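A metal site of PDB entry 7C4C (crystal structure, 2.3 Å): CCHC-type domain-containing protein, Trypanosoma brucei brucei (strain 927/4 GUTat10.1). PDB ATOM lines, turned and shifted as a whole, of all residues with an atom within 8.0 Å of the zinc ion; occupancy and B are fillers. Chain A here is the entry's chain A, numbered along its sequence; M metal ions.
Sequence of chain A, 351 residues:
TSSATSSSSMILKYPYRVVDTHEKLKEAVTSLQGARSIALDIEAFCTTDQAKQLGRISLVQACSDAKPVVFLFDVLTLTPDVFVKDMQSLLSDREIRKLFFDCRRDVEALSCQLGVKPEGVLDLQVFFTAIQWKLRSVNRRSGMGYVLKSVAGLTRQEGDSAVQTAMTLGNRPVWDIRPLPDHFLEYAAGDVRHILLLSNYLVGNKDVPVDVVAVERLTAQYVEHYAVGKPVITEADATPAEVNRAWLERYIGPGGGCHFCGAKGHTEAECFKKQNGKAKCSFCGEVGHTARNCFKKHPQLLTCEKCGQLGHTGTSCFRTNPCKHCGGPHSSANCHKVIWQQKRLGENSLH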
ATOM      1  N   PRO A 322       8.080  26.721  13.088  1.00  0.00           N
ATOM      2  CA  PRO A 322       7.489  26.828  14.412  1.00  0.00           C
ATOM      3  C   PRO A 322       6.605  28.050  14.618  1.00  0.00           C
ATOM      4  O   PRO A 322       6.573  28.943  13.800  1.00  0.00           O
ATOM      5  CB  PRO A 322       8.689  26.896  15.337  1.00  0.00           C
ATOM      6  CG  PRO A 322       9.880  26.837  14.468  1.00  0.00           C
ATOM      7  CD  PRO A 322       9.452  26.218  13.185  1.00  0.00           C
ATOM      8  N   CYS A 323       5.851  28.053  15.698  1.00  0.00           N
ATOM      9  CA  CYS A 323       4.897  29.115  15.989  1.00  0.00           C
ATOM     10  C   CYS A 323       5.414  30.532  16.149  1.00  0.00           C
ATOM     11  O   CYS A 323       6.343  30.793  16.858  1.00  0.00           O
ATOM     12  CB  CYS A 323       4.042  28.765  17.210  1.00  0.00           C
ATOM     13  SG  CYS A 323       2.569  29.784  17.344  1.00  0.00           S
ATOM     14  N   LYS A 324       4.659  31.431  15.534  1.00  0.00           N
ATOM     15  CA  LYS A 324       4.877  32.862  15.481  1.00  0.00           C
ATOM     16  C   LYS A 324       4.847  33.465  16.857  1.00  0.00           C
ATOM     17  O   LYS A 324       5.593  34.360  17.154  1.00  0.00           O
ATOM     18  CB  LYS A 324       3.737  33.487  14.674  1.00  0.00           C
ATOM     19  CG  LYS A 324       3.898  34.912  14.193  1.00  0.00           C
ATOM     20  CD  LYS A 324       2.808  35.254  13.192  1.00  0.00           C
ATOM     21  CE  LYS A 324       1.872  36.347  13.696  1.00  0.00           C
ATOM     22  NZ  LYS A 324       0.953  36.937  12.673  1.00  0.00           N
ATOM     23  N   HIS A 325       3.931  32.959  17.683  1.00  0.00           N
ATOM     24  CA  HIS A 325       3.685  33.403  19.040  1.00  0.00           C
ATOM     25  C   HIS A 325       4.594  32.935  20.196  1.00  0.00           C
ATOM     26  O   HIS A 325       4.811  33.723  21.081  1.00  0.00           O
ATOM     27  CB  HIS A 325       2.184  33.350  19.223  1.00  0.00           C
ATOM     28  CG  HIS A 325       1.438  33.980  18.098  1.00  0.00           C
ATOM     29  ND1 HIS A 325       0.377  33.367  17.474  1.00  0.00           N
ATOM     30  CD2 HIS A 325       1.606  35.159  17.472  1.00  0.00           C
ATOM     31  CE1 HIS A 325      -0.078  34.146  16.515  1.00  0.00           C
ATOM     32  NE2 HIS A 325       0.654  35.245  16.501  1.00  0.00           N
ATOM     33  N   CYS A 326       4.875  31.635  20.235  1.00  0.00           N
ATOM     34  CA  CYS A 326       5.637  30.973  21.296  1.00  0.00           C
ATOM     35  C   CYS A 326       6.784  30.051  20.911  1.00  0.00           C
ATOM     36  O   CYS A 326       7.500  29.570  21.752  1.00  0.00           O
ATOM     37  CB  CYS A 326       4.647  30.098  22.095  1.00  0.00           C
ATOM     38  SG  CYS A 326       3.875  28.680  21.251  1.00  0.00           S
ATOM     39  N   GLY A 327       6.854  29.729  19.630  1.00  0.00           N
ATOM     40  CA  GLY A 327       7.839  28.808  19.107  1.00  0.00           C
ATOM     41  C   GLY A 327       7.503  27.344  19.260  1.00  0.00           C
ATOM     42  O   GLY A 327       8.309  26.507  19.013  1.00  0.00           O
ATOM     43  N   GLY A 328       6.282  27.045  19.668  1.00  0.00           N
ATOM     44  CA  GLY A 328       5.774  25.694  19.919  1.00  0.00           C
ATOM     45  C   GLY A 328       5.443  24.796  18.746  1.00  0.00           C
ATOM     46  O   GLY A 328       5.399  25.252  17.615  1.00  0.00           O
ATOM     47  N   PRO A 329       5.167  23.529  19.021  1.00  0.00           N
ATOM     48  CA  PRO A 329       4.904  22.527  17.977  1.00  0.00           C
ATOM     49  C   PRO A 329       3.517  22.498  17.366  1.00  0.00           C
ATOM     50  O   PRO A 329       2.765  21.562  17.495  1.00  0.00           O
ATOM     51  CB  PRO A 329       5.155  21.199  18.692  1.00  0.00           C
ATOM     52  CG  PRO A 329       5.579  21.502  20.084  1.00  0.00           C
ATOM     53  CD  PRO A 329       5.902  22.954  20.156  1.00  0.00           C
ATOM     54  N   HIS A 330       3.251  23.549  16.640  1.00  0.00           N
ATOM     55  CA  HIS A 330       2.041  23.770  15.864  1.00  0.00           C
ATOM     56  C   HIS A 330       2.114  25.062  15.042  1.00  0.00           C
ATOM     57  O   HIS A 330       3.129  25.775  15.029  1.00  0.00           O
ATOM     58  CB  HIS A 330       0.810  23.862  16.763  1.00  0.00           C
ATOM     59  CG  HIS A 330       0.906  24.898  17.847  1.00  0.00           C
ATOM     60  ND1 HIS A 330       1.659  24.701  18.978  1.00  0.00           N
ATOM     61  CD2 HIS A 330       0.338  26.120  17.980  1.00  0.00           C
ATOM     62  CE1 HIS A 330       1.568  25.753  19.754  1.00  0.00           C
ATOM     63  NE2 HIS A 330       0.771  26.635  19.176  1.00  0.00           N
ATOM     64  N   SER A 331       1.001  25.386  14.367  1.00  0.00           N
ATOM     65  CA  SER A 331       0.889  26.538  13.487  1.00  0.00           C
ATOM     66  C   SER A 331       0.394  27.747  14.267  1.00  0.00           C
ATOM     67  O   SER A 331      -0.180  27.626  15.353  1.00  0.00           O
ATOM     68  CB  SER A 331      -0.055  26.238  12.320  1.00  0.00           C
ATOM     69  OG  SER A 331      -1.412  26.200  12.749  1.00  0.00           O
ATOM     70  N   SER A 332       0.608  28.930  13.678  1.00  0.00           N
ATOM     71  CA  SER A 332       0.393  30.180  14.394  1.00  0.00           C
ATOM     72  C   SER A 332      -1.088  30.486  14.596  1.00  0.00           C
ATOM     73  O   SER A 332      -1.474  31.059  15.625  1.00  0.00           O
ATOM     74  CB  SER A 332       1.068  31.329  13.637  1.00  0.00           C
ATOM     75  OG  SER A 332       2.422  31.008  13.314  1.00  0.00           O
ATOM     76  N   ALA A 333      -1.928  30.123  13.630  1.00  0.00           N
ATOM     77  CA  ALA A 333      -3.342  30.494  13.721  1.00  0.00           C
ATOM     78  C   ALA A 333      -4.031  29.799  14.887  1.00  0.00           C
ATOM     79  O   ALA A 333      -4.928  30.379  15.497  1.00  0.00           O
ATOM     80  CB  ALA A 333      -4.053  30.184  12.408  1.00  0.00           C
ATOM     81  N   ASN A 334      -3.624  28.565  15.213  1.00  0.00           N
ATOM     82  CA  ASN A 334      -4.249  27.769  16.261  1.00  0.00           C
ATOM     83  C   ASN A 334      -3.546  27.878  17.614  1.00  0.00           C
ATOM     84  O   ASN A 334      -3.907  27.141  18.541  1.00  0.00           O
ATOM     85  CB  ASN A 334      -4.315  26.272  15.877  1.00  0.00           C
ATOM     86  CG  ASN A 334      -4.452  26.043  14.366  1.00  0.00           C
ATOM     87  OD1 ASN A 334      -3.502  25.621  13.709  1.00  0.00           O
ATOM     88  ND2 ASN A 334      -5.632  26.315  13.822  1.00  0.00           N
ATOM     89  N   CYS A 335      -2.544  28.768  17.756  1.00  0.00           N
ATOM     90  CA  CYS A 335      -1.959  29.024  19.067  1.00  0.00           C
ATOM     91  C   CYS A 335      -3.013  29.529  20.043  1.00  0.00           C
ATOM     92  O   CYS A 335      -3.852  30.364  19.691  1.00  0.00           O
ATOM     93  CB  CYS A 335      -0.814  30.056  18.944  1.00  0.00           C
ATOM     94  SG  CYS A 335       0.106  30.386  20.491  1.00  0.00           S
ATOM     95  N   HIS A 336      -2.978  29.013  21.264  1.00  0.00           N
ATOM     96  CA  HIS A 336      -4.014  29.358  22.237  1.00  0.00           C
ATOM     97  C   HIS A 336      -3.889  30.776  22.765  1.00  0.00           C
ATOM     98  O   HIS A 336      -4.759  31.222  23.523  1.00  0.00           O
ATOM     99  CB  HIS A 336      -3.994  28.375  23.405  1.00  0.00           C
ATOM    100  CG  HIS A 336      -2.717  28.375  24.178  1.00  0.00           C
ATOM    101  ND1 HIS A 336      -1.569  27.746  23.728  1.00  0.00           N
ATOM    102  CD2 HIS A 336      -2.403  28.920  25.382  1.00  0.00           C
ATOM    103  CE1 HIS A 336      -0.599  27.914  24.611  1.00  0.00           C
ATOM    104  NE2 HIS A 336      -1.078  28.620  25.625  1.00  0.00           N
ATOM    105  N   LYS A 337      -2.823  31.495  22.381  1.00  0.00           N
ATOM    106  CA  LYS A 337      -2.628  32.882  22.781  1.00  0.00           C
ATOM    107  C   LYS A 337      -3.462  33.845  21.939  1.00  0.00           C
ATOM    108  O   LYS A 337      -3.887  34.891  22.439  1.00  0.00           O
ATOM    109  CB  LYS A 337      -1.145  33.241  22.702  1.00  0.00           C
ATOM    110  CG  LYS A 337      -0.235  32.355  23.554  1.00  0.00           C
ATOM    111  CD  LYS A 337       1.236  32.560  23.200  1.00  0.00           C
ATOM    112  CE  LYS A 337       1.927  33.507  24.175  1.00  0.00           C
ATOM    113  NZ  LYS A 337       3.418  33.284  24.176  1.00  0.00           N
ATOM    114  N   VAL A 338      -3.706  33.514  20.662  1.00  0.00           N
ATOM    115  CA  VAL A 338      -4.464  34.390  19.764  1.00  0.00           C
ATOM    116  C   VAL A 338      -5.915  33.919  19.661  1.00  0.00           C
ATOM    117  O   VAL A 338      -6.841  34.735  19.585  1.00  0.00           O
ATOM    118  CB  VAL A 338      -3.796  34.495  18.378  1.00  0.00           C
ATOM    119  CG1 VAL A 338      -2.336  34.925  18.499  1.00  0.00           C
ATOM    120  CG2 VAL A 338      -3.886  33.175  17.605  1.00  0.00           C
HETATM  121 ZN    ZN M   1       1.858  29.045  19.845  1.00  0.00          ZN
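N of Cys 323 is in hydrogen-bond range of O of Gly 328.
SG of Cys 335 lies close to N of Lys 337, at 3.7 Å.
The side-chain sulfur (SG) of Cys 323 lies close to the backbone NH (N) of His 325.
The side-chain sulfur (SG) of Cys 326 sits close to the backbone NH (N) of Gly 328 (3.3 Å).
Within 4 Å of the zinc ion: Cys 323, Cys 326, His 330 and Cys 335.
The zinc ion is bound by the side-chain sulfur of Cys 335 (2.3 Å), the side-chain sulfur of Cys 326 (2.5 Å) and the side-chain sulfur of Cys 323 (2.7 Å).
The zinc ion has three donor atoms within binding distance.
Slightly farther from the zinc ion lies NE2 of His 330 (2.7 Å).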
